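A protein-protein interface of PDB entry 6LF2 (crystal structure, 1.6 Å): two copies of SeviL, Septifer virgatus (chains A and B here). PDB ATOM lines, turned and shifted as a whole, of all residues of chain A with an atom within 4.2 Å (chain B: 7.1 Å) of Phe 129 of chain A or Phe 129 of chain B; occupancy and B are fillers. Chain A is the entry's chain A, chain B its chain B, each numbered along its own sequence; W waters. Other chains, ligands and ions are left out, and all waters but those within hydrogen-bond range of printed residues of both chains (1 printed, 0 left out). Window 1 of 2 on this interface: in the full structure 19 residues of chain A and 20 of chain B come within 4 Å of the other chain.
Water W1 lies within hydrogen-bond range of NH2 of Arg 22 of chain B (2.8 Å), NE2 of Gln 15 of chain A (3.2 Å) and OE1 of Gln 15 of chain B (3.3 Å).
OH of Tyr 13 of chain A touches CE1 of Phe 95 of chain B, 3.6 Å away.
Gln 15 of chain A touches Arg 22 of chain B (NE2 to NE, 3.7 Å).
Met 39 of chain A touches Ile 127 of chain B (SD to CG2, 3.9 Å).
Met 39 of chain B touches Ile 127 of chain A (SD to CG2, 3.9 Å).
Ile 127 of chain A touches Lys 130 of chain B.
Ile 127 of chain A touches Ala 131 of chain B (CD1 to O, 3.96 Å).
CE1 of Phe 129 of chain A touches CD1 of Ile 127 of chain B, at 3.9 Å.
Phe 129 of chain B touches Phe 129 of chain A (CG to CD1, 3.4 Å).
CD1 of Ile 127 of chain B touches O of Lys 130 of chain A, 3.8 Å away.
Ile 127 of chain B touches Ala 131 of chain A.
NE2 of Gln 15 of chain A lies within hydrogen-bond range of OE1 of Gln 15 of chain B.
The side-chain amide nitrogen of Gln 15 of chain A is in hydrogen-bond range of the side-chain sulfur of Met 39 of chain B, at 3.5 Å.
The side-chain amide nitrogen of Gln 15 of chain B is in hydrogen-bond range of the side-chain sulfur of Met 39 of chain A.
Of the 15 printed residues of chain B, 8 touch a printed residue of chain A.
Printed residues of chain B that touch a printed residue of chain A: Gln 15, Arg 22, Met 39, Phe 95, Ile 127, Phe 129, Lys 130 and Ala 131.
Hydrophobic or aromatic side chains of chain B that line the printed part of chain A: Met 39, Phe 95, Ile 127 and Phe 129.
Hydrophobic or aromatic side chains of chain A that line the printed part of chain B: Tyr 13, Met 39, Ile 127 and Phe 129.
Among the printed residues, no Asp or Glu carboxylate lies within 4 Å of a Lys or Arg side-chain nitrogen of the other chain.
The backbone NH (N) of Tyr 13 of chain A is in hydrogen-bond range of the backbone carbonyl oxygen (O) of Phe 129 of chain A (2.9 Å).
O of Gln 15 of chain A is in hydrogen-bond range of N of Ile 127 of chain A, 2.8 Å away.
O of Lys 11 of chain B lies within hydrogen-bond range of N of Ala 131 of chain B (2.9 Å).
O of Phe 129 of chain B is in hydrogen-bond range of N of Tyr 13 of chain B (2.9 Å).
The guanidinium group (NE) of Arg 22 of chain B lies within hydrogen-bond range of the side-chain amide oxygen (OE1) of Gln 15 of chain B, 2.9 Å away.
The backbone NH (N) of Ile 127 of chain B is in hydrogen-bond range of the backbone carbonyl oxygen (O) of Gln 15 of chain B, 2.8 Å away.
Printed residues of chain A within 4 Å of Gln 15 of chain B: Gln 15 and Met 39.
Trp 45 of chain B touches none of the printed residues of chain A.
Of the printed residues of chain A, Phe 95 of chain B touches Tyr 13 (3.6 Å).
Of chain A, only Ile 127 and Phe 129 come within 4 Å of Phe 129 of chain B.
The nearest printed residue of chain A that does not touch Phe 129 of chain B is Gln 15 of chain A (4.3 Å).
The nearest printed residue of chain A that does not touch Phe 95 of chain B is Met 39 of chain A (4.001 Å).
Tyr 13 of chain A touches Ile 127 of chain B, but with the chains exchanged Ile 127 of chain A does not touch Tyr 13 of chain B (4.02 Å).
Ile 127 of chain A touches Lys 130 of chain B, and with the chains exchanged Lys 130 of chain A touches Ile 127 of chain B.
Ile 127 of chain A touches Ala 131 of chain B, and with the chains exchanged Ala 131 of chain A touches Ile 127 of chain B.
Phe 129 of chain B touches its own counterpart, Phe 129 of chain A.
9 positions are printed for both chains.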
ATOM      1  N   CYS A  12     -19.020   1.076  -7.564  1.00  0.00           N
ATOM      2  CA  CYS A  12     -18.115   1.054  -8.701  1.00  0.00           C
ATOM      3  C   CYS A  12     -16.748   0.518  -8.296  1.00  0.00           C
ATOM      4  O   CYS A  12     -16.396   0.455  -7.114  1.00  0.00           O
ATOM      5  CB  CYS A  12     -17.951   2.444  -9.304  1.00  0.00           C
ATOM      6  SG  CYS A  12     -17.261   3.614  -8.122  1.00  0.00           S
ATOM      7  N   TYR A  13     -15.978   0.136  -9.309  1.00  0.00           N
ATOM      8  CA  TYR A  13     -14.548  -0.095  -9.177  1.00  0.00           C
ATOM      9  C   TYR A  13     -13.822   1.136  -9.696  1.00  0.00           C
ATOM     10  O   TYR A  13     -14.322   1.835 -10.579  1.00  0.00           O
ATOM     11  CB  TYR A  13     -14.104  -1.325  -9.980  1.00  0.00           C
ATOM     12  CG  TYR A  13     -14.706  -2.635  -9.522  1.00  0.00           C
ATOM     13  CD1 TYR A  13     -14.116  -3.362  -8.492  1.00  0.00           C
ATOM     14  CD2 TYR A  13     -15.843  -3.163 -10.141  1.00  0.00           C
ATOM     15  CE1 TYR A  13     -14.653  -4.568  -8.062  1.00  0.00           C
ATOM     16  CE2 TYR A  13     -16.397  -4.386  -9.711  1.00  0.00           C
ATOM     17  CZ  TYR A  13     -15.782  -5.086  -8.683  1.00  0.00           C
ATOM     18  OH  TYR A  13     -16.292  -6.288  -8.228  1.00  0.00           O
ATOM     19  N   GLN A  15     -10.239   2.076 -11.227  1.00  0.00           N
ATOM     20  CA  GLN A  15      -9.139   1.339 -11.834  1.00  0.00           C
ATOM     21  C   GLN A  15      -8.212   2.277 -12.596  1.00  0.00           C
ATOM     22  O   GLN A  15      -8.669   3.183 -13.297  1.00  0.00           O
ATOM     23  CB  GLN A  15      -9.682   0.264 -12.779  1.00  0.00           C
ATOM     24  CG  GLN A  15      -8.615  -0.611 -13.378  1.00  0.00           C
ATOM     25  CD  GLN A  15      -9.186  -1.923 -13.858  1.00  0.00           C
ATOM     26  OE1 GLN A  15      -9.708  -2.700 -13.065  1.00  0.00           O
ATOM     27  NE2 GLN A  15      -9.107  -2.168 -15.162  1.00  0.00           N
ATOM     28  N   MET A  39     -10.189  -9.446  -8.400  1.00  0.00           N
ATOM     29  CA  MET A  39     -11.162  -8.387  -8.115  1.00  0.00           C
ATOM     30  C   MET A  39     -11.928  -8.719  -6.836  1.00  0.00           C
ATOM     31  O   MET A  39     -13.063  -9.193  -6.858  1.00  0.00           O
ATOM     32  CB  MET A  39     -12.108  -8.204  -9.298  1.00  0.00           C
ATOM     33  CG  MET A  39     -11.388  -7.915 -10.603  1.00  0.00           C
ATOM     34  SD  MET A  39     -12.498  -7.477 -11.958  1.00  0.00           S
ATOM     35  CE  MET A  39     -13.185  -5.932 -11.348  1.00  0.00           C
ATOM     36  N   ILE A 127     -10.519   4.955 -14.445  1.00  0.00           N
ATOM     37  CA  ILE A 127     -11.839   4.650 -14.981  1.00  0.00           C
ATOM     38  C   ILE A 127     -12.690   4.107 -13.840  1.00  0.00           C
ATOM     39  O   ILE A 127     -12.261   3.214 -13.101  1.00  0.00           O
ATOM     40  CB  ILE A 127     -11.756   3.686 -16.183  1.00  0.00           C
ATOM     41  CG1 ILE A 127     -13.149   3.402 -16.750  1.00  0.00           C
ATOM     42  CG2 ILE A 127     -10.975   2.411 -15.844  1.00  0.00           C
ATOM     43  CD1 ILE A 127     -13.097   2.885 -18.177  1.00  0.00           C
ATOM     44  N   LEU A 128     -13.868   4.691 -13.653  1.00  0.00           N
ATOM     45  CA  LEU A 128     -14.760   4.314 -12.562  1.00  0.00           C
ATOM     46  C   LEU A 128     -15.940   3.593 -13.195  1.00  0.00           C
ATOM     47  O   LEU A 128     -16.788   4.233 -13.827  1.00  0.00           O
ATOM     48  CB  LEU A 128     -15.221   5.539 -11.768  1.00  0.00           C
ATOM     49  CG  LEU A 128     -14.115   6.343 -11.067  1.00  0.00           C
ATOM     50  CD1 LEU A 128     -13.460   7.348 -12.005  1.00  0.00           C
ATOM     51  CD2 LEU A 128     -14.677   7.033  -9.821  1.00  0.00           C
ATOM     52  N   PHE A 129     -15.987   2.269 -13.055  1.00  0.00           N
ATOM     53  CA  PHE A 129     -17.003   1.496 -13.753  1.00  0.00           C
ATOM     54  C   PHE A 129     -17.945   0.775 -12.796  1.00  0.00           C
ATOM     55  O   PHE A 129     -17.581   0.388 -11.683  1.00  0.00           O
ATOM     56  CB  PHE A 129     -16.375   0.507 -14.768  1.00  0.00           C
ATOM     57  CG  PHE A 129     -15.419  -0.514 -14.181  1.00  0.00           C
ATOM     58  CD1 PHE A 129     -15.874  -1.780 -13.819  1.00  0.00           C
ATOM     59  CD2 PHE A 129     -14.052  -0.252 -14.086  1.00  0.00           C
ATOM     60  CE1 PHE A 129     -14.991  -2.749 -13.335  1.00  0.00           C
ATOM     61  CE2 PHE A 129     -13.177  -1.209 -13.585  1.00  0.00           C
ATOM     62  CZ  PHE A 129     -13.644  -2.465 -13.226  1.00  0.00           C
ATOM     63  N   LYS A 130     -19.183   0.619 -13.255  1.00  0.00           N
ATOM     64  CA  LYS A 130     -20.252   0.082 -12.428  1.00  0.00           C
ATOM     65  C   LYS A 130     -19.896  -1.302 -11.902  1.00  0.00           C
ATOM     66  O   LYS A 130     -19.450  -2.169 -12.661  1.00  0.00           O
ATOM     67  CB  LYS A 130     -21.547   0.023 -13.243  1.00  0.00           C
ATOM     68  CG  LYS A 130     -22.014   1.384 -13.748  1.00  0.00           C
ATOM     69  CD  LYS A 130     -23.503   1.384 -14.111  1.00  0.00           C
ATOM     70  CE  LYS A 130     -24.334   2.223 -13.125  1.00  0.00           C
ATOM     71  NZ  LYS A 130     -24.065   3.697 -13.219  1.00  0.00           N
ATOM     72  N   ALA A 131     -20.098  -1.511 -10.599  1.00  0.00           N
ATOM     73  CA  ALA A 131     -19.731  -2.798 -10.007  1.00  0.00           C
ATOM     74  C   ALA A 131     -20.805  -3.847 -10.244  1.00  0.00           C
ATOM     75  O   ALA A 131     -20.491  -5.020 -10.470  1.00  0.00           O
ATOM     76  CB  ALA A 131     -19.469  -2.645  -8.511  1.00  0.00           C
ATOM     77  N   LYS B  11     -19.625  -0.204 -26.305  1.00  0.00           N
ATOM     78  CA  LYS B  11     -18.204  -0.510 -26.331  1.00  0.00           C
ATOM     79  C   LYS B  11     -17.781  -0.838 -24.910  1.00  0.00           C
ATOM     80  O   LYS B  11     -18.150  -0.117 -23.978  1.00  0.00           O
ATOM     81  CB  LYS B  11     -17.397   0.676 -26.866  1.00  0.00           C
ATOM     82  CG  LYS B  11     -17.653   1.033 -28.332  1.00  0.00           C
ATOM     83  CD  LYS B  11     -16.904   0.116 -29.292  1.00  0.00           C
ATOM     84  CE  LYS B  11     -17.270   0.433 -30.733  1.00  0.00           C
ATOM     85  NZ  LYS B  11     -17.105   1.881 -31.040  1.00  0.00           N
ATOM     86  N   CYS B  12     -17.020  -1.917 -24.737  1.00  0.00           N
ATOM     87  CA  CYS B  12     -16.751  -2.366 -23.381  1.00  0.00           C
ATOM     88  C   CYS B  12     -15.386  -3.025 -23.254  1.00  0.00           C
ATOM     89  O   CYS B  12     -14.837  -3.574 -24.213  1.00  0.00           O
ATOM     90  CB  CYS B  12     -17.829  -3.338 -22.894  1.00  0.00           C
ATOM     91  SG  CYS B  12     -17.867  -4.901 -23.784  1.00  0.00           S
ATOM     92  N   TYR B  13     -14.844  -2.960 -22.039  1.00  0.00           N
ATOM     93  CA  TYR B  13     -13.749  -3.832 -21.656  1.00  0.00           C
ATOM     94  C   TYR B  13     -14.334  -5.132 -21.123  1.00  0.00           C
ATOM     95  O   TYR B  13     -15.454  -5.157 -20.602  1.00  0.00           O
ATOM     96  CB  TYR B  13     -12.867  -3.193 -20.580  1.00  0.00           C
ATOM     97  CG  TYR B  13     -12.144  -1.934 -21.013  1.00  0.00           C
ATOM     98  CD1 TYR B  13     -10.883  -2.002 -21.577  1.00  0.00           C
ATOM     99  CD2 TYR B  13     -12.722  -0.672 -20.833  1.00  0.00           C
ATOM    100  CE1 TYR B  13     -10.205  -0.851 -21.975  1.00  0.00           C
ATOM    101  CE2 TYR B  13     -12.055   0.483 -21.227  1.00  0.00           C
ATOM    102  CZ  TYR B  13     -10.802   0.385 -21.792  1.00  0.00           C
ATOM    103  OH  TYR B  13     -10.120   1.510 -22.197  1.00  0.00           O
ATOM    104  N   ILE B  14     -13.578  -6.214 -21.279  1.00  0.00           N
ATOM    105  CA  ILE B  14     -13.996  -7.553 -20.867  1.00  0.00           C
ATOM    106  C   ILE B  14     -12.913  -8.063 -19.923  1.00  0.00           C
ATOM    107  O   ILE B  14     -11.834  -8.481 -20.354  1.00  0.00           O
ATOM    108  CB  ILE B  14     -14.216  -8.488 -22.065  1.00  0.00           C
ATOM    109  CG1 ILE B  14     -15.291  -7.892 -22.983  1.00  0.00           C
ATOM    110  CG2 ILE B  14     -14.617  -9.886 -21.585  1.00  0.00           C
ATOM    111  CD1 ILE B  14     -15.555  -8.677 -24.272  1.00  0.00           C
ATOM    112  N   GLN B  15     -13.181  -7.993 -18.619  1.00  0.00           N
ATOM    113  CA  GLN B  15     -12.156  -8.172 -17.604  1.00  0.00           C
ATOM    114  C   GLN B  15     -12.486  -9.360 -16.707  1.00  0.00           C
ATOM    115  O   GLN B  15     -13.651  -9.592 -16.370  1.00  0.00           O
ATOM    116  CB  GLN B  15     -12.015  -6.885 -16.772  1.00  0.00           C
ATOM    117  CG  GLN B  15     -10.911  -6.931 -15.720  1.00  0.00           C
ATOM    118  CD  GLN B  15     -10.524  -5.545 -15.241  1.00  0.00           C
ATOM    119  OE1 GLN B  15     -10.096  -4.694 -16.034  1.00  0.00           O
ATOM    120  NE2 GLN B  15     -10.670  -5.310 -13.935  1.00  0.00           N
ATOM    121  N   ARG B  22      -7.613  -8.232 -18.963  1.00  0.00           N
ATOM    122  CA  ARG B  22      -8.555  -7.807 -19.987  1.00  0.00           C
ATOM    123  C   ARG B  22      -8.288  -8.561 -21.284  1.00  0.00           C
ATOM    124  O   ARG B  22      -7.135  -8.683 -21.711  1.00  0.00           O
ATOM    125  CB  ARG B  22      -8.474  -6.290 -20.216  1.00  0.00           C
ATOM    126  CG  ARG B  22      -9.327  -5.470 -19.242  1.00  0.00           C
ATOM    127  CD  ARG B  22      -8.620  -4.197 -18.767  1.00  0.00           C
ATOM    128  NE  ARG B  22      -7.713  -4.486 -17.653  1.00  0.00           N
ATOM    129  CZ  ARG B  22      -6.392  -4.343 -17.687  1.00  0.00           C
ATOM    130  NH1 ARG B  22      -5.782  -3.896 -18.777  1.00  0.00           N
ATOM    131  NH2 ARG B  22      -5.670  -4.650 -16.613  1.00  0.00           N
ATOM    132  N   MET B  39      -3.959  -0.495 -19.419  1.00  0.00           N
ATOM    133  CA  MET B  39      -5.145  -0.483 -20.267  1.00  0.00           C
ATOM    134  C   MET B  39      -4.799   0.137 -21.618  1.00  0.00           C
ATOM    135  O   MET B  39      -4.279   1.259 -21.688  1.00  0.00           O
ATOM    136  CB  MET B  39      -6.273   0.277 -19.565  1.00  0.00           C
ATOM    137  CG  MET B  39      -6.606  -0.319 -18.187  1.00  0.00           C
ATOM    138  SD  MET B  39      -8.042   0.391 -17.352  1.00  0.00           S
ATOM    139  CE  MET B  39      -9.361  -0.098 -18.459  1.00  0.00           C
ATOM    140  N   TRP B  45     -13.935  -3.617 -26.872  1.00  0.00           N
ATOM    141  CA  TRP B  45     -14.705  -4.481 -27.759  1.00  0.00           C
ATOM    142  C   TRP B  45     -16.063  -3.875 -28.065  1.00  0.00           C
ATOM    143  O   TRP B  45     -16.631  -3.133 -27.258  1.00  0.00           O
ATOM    144  CB  TRP B  45     -14.927  -5.877 -27.142  1.00  0.00           C
ATOM    145  CG  TRP B  45     -13.661  -6.609 -26.830  1.00  0.00           C
ATOM    146  CD1 TRP B  45     -12.853  -6.411 -25.744  1.00  0.00           C
ATOM    147  CD2 TRP B  45     -13.047  -7.667 -27.592  1.00  0.00           C
ATOM    148  NE1 TRP B  45     -11.785  -7.261 -25.789  1.00  0.00           N
ATOM    149  CE2 TRP B  45     -11.873  -8.045 -26.908  1.00  0.00           C
ATOM    150  CE3 TRP B  45     -13.371  -8.325 -28.787  1.00  0.00           C
ATOM    151  CZ2 TRP B  45     -11.021  -9.051 -27.367  1.00  0.00           C
ATOM    152  CZ3 TRP B  45     -12.518  -9.327 -29.245  1.00  0.00           C
ATOM    153  CH2 TRP B  45     -11.361  -9.683 -28.538  1.00  0.00           C
ATOM    154  N   PHE B  95     -20.954 -10.019 -12.403  1.00  0.00           N
ATOM    155  CA  PHE B  95     -20.119 -10.876 -13.230  1.00  0.00           C
ATOM    156  C   PHE B  95     -20.959 -11.872 -14.019  1.00  0.00           C
ATOM    157  O   PHE B  95     -22.056 -12.260 -13.607  1.00  0.00           O
ATOM    158  CB  PHE B  95     -19.087 -11.617 -12.377  1.00  0.00           C
ATOM    159  CG  PHE B  95     -18.005 -10.712 -11.847  1.00  0.00           C
ATOM    160  CD1 PHE B  95     -18.201  -9.996 -10.683  1.00  0.00           C
ATOM    161  CD2 PHE B  95     -16.814 -10.548 -12.541  1.00  0.00           C
ATOM    162  CE1 PHE B  95     -17.220  -9.154 -10.199  1.00  0.00           C
ATOM    163  CE2 PHE B  95     -15.829  -9.696 -12.058  1.00  0.00           C
ATOM    164  CZ  PHE B  95     -16.037  -9.003 -10.885  1.00  0.00           C
ATOM    165  N   ILE B 127     -16.402  -9.383 -16.034  1.00  0.00           N
ATOM    166  CA  ILE B 127     -17.184  -8.167 -15.929  1.00  0.00           C
ATOM    167  C   ILE B 127     -16.948  -7.376 -17.212  1.00  0.00           C
ATOM    168  O   ILE B 127     -15.800  -7.161 -17.620  1.00  0.00           O
ATOM    169  CB  ILE B 127     -16.821  -7.375 -14.657  1.00  0.00           C
ATOM    170  CG1 ILE B 127     -17.688  -6.116 -14.532  1.00  0.00           C
ATOM    171  CG2 ILE B 127     -15.327  -7.073 -14.608  1.00  0.00           C
ATOM    172  CD1 ILE B 127     -17.734  -5.560 -13.109  1.00  0.00           C
ATOM    173  N   LEU B 128     -18.035  -7.023 -17.886  1.00  0.00           N
ATOM    174  CA  LEU B 128     -17.995  -6.316 -19.158  1.00  0.00           C
ATOM    175  C   LEU B 128     -18.463  -4.900 -18.868  1.00  0.00           C
ATOM    176  O   LEU B 128     -19.654  -4.672 -18.653  1.00  0.00           O
ATOM    177  CB  LEU B 128     -18.891  -6.990 -20.196  1.00  0.00           C
ATOM    178  CG  LEU B 128     -18.552  -8.429 -20.589  1.00  0.00           C
ATOM    179  CD1 LEU B 128     -19.203  -9.418 -19.639  1.00  0.00           C
ATOM    180  CD2 LEU B 128     -19.028  -8.671 -22.014  1.00  0.00           C
ATOM    181  N   PHE B 129     -17.527  -3.955 -18.805  1.00  0.00           N
ATOM    182  CA  PHE B 129     -17.878  -2.612 -18.374  1.00  0.00           C
ATOM    183  C   PHE B 129     -17.667  -1.590 -19.485  1.00  0.00           C
ATOM    184  O   PHE B 129     -16.794  -1.742 -20.340  1.00  0.00           O
ATOM    185  CB  PHE B 129     -17.110  -2.196 -17.102  1.00  0.00           C
ATOM    186  CG  PHE B 129     -15.593  -2.196 -17.228  1.00  0.00           C
ATOM    187  CD1 PHE B 129     -14.917  -1.031 -17.584  1.00  0.00           C
ATOM    188  CD2 PHE B 129     -14.844  -3.319 -16.890  1.00  0.00           C
ATOM    189  CE1 PHE B 129     -13.546  -0.994 -17.653  1.00  0.00           C
ATOM    190  CE2 PHE B 129     -13.464  -3.292 -16.957  1.00  0.00           C
ATOM    191  CZ  PHE B 129     -12.806  -2.123 -17.335  1.00  0.00           C
ATOM    192  N   LYS B 130     -18.507  -0.552 -19.450  1.00  0.00           N
ATOM    193  CA  LYS B 130     -18.517   0.490 -20.471  1.00  0.00           C
ATOM    194  C   LYS B 130     -17.146   1.130 -20.618  1.00  0.00           C
ATOM    195  O   LYS B 130     -16.540   1.545 -19.628  1.00  0.00           O
ATOM    196  CB  LYS B 130     -19.540   1.563 -20.100  1.00  0.00           C
ATOM    197  CG  LYS B 130     -20.963   1.061 -20.005  1.00  0.00           C
ATOM    198  CD  LYS B 130     -21.901   2.146 -19.505  1.00  0.00           C
ATOM    199  CE  LYS B 130     -23.304   1.588 -19.319  1.00  0.00           C
ATOM    200  NZ  LYS B 130     -23.301   0.333 -18.513  1.00  0.00           N
ATOM    201  N   ALA B 131     -16.660   1.226 -21.859  1.00  0.00           N
ATOM    202  CA  ALA B 131     -15.356   1.843 -22.097  1.00  0.00           C
ATOM    203  C   ALA B 131     -15.418   3.367 -22.085  1.00  0.00           C
ATOM    204  O   ALA B 131     -14.426   4.016 -21.730  1.00  0.00           O
ATOM    205  CB  ALA B 131     -14.770   1.369 -23.430  1.00  0.00           C
ATOM    206  N   TYR B 132     -16.551   3.949 -22.478  1.00  0.00           N
ATOM    207  CA  TYR B 132     -16.687   5.399 -22.638  1.00  0.00           C
ATOM    208  C   TYR B 132     -17.824   5.954 -21.784  1.00  0.00           C
ATOM    209  O   TYR B 132     -17.936   7.165 -21.601  1.00  0.00           O
ATOM    210  CB  TYR B 132     -16.956   5.782 -24.100  1.00  0.00           C
ATOM    211  CG  TYR B 132     -16.005   5.208 -25.120  1.00  0.00           C
ATOM    212  CD1 TYR B 132     -14.675   4.990 -24.816  1.00  0.00           C
ATOM    213  CD2 TYR B 132     -16.445   4.891 -26.397  1.00  0.00           C
ATOM    214  CE1 TYR B 132     -13.809   4.464 -25.751  1.00  0.00           C
ATOM    215  CE2 TYR B 132     -15.590   4.368 -27.337  1.00  0.00           C
ATOM    216  CZ  TYR B 132     -14.271   4.155 -27.010  1.00  0.00           C
ATOM    217  OH  TYR B 132     -13.403   3.634 -27.944  1.00  0.00           O
ATOM    218  OXT TYR B 132     -18.678   5.219 -21.285  1.00  0.00           O
HETATM  219  O   HOH W   1      -7.277  -4.666 -14.354  1.00  0.00           O
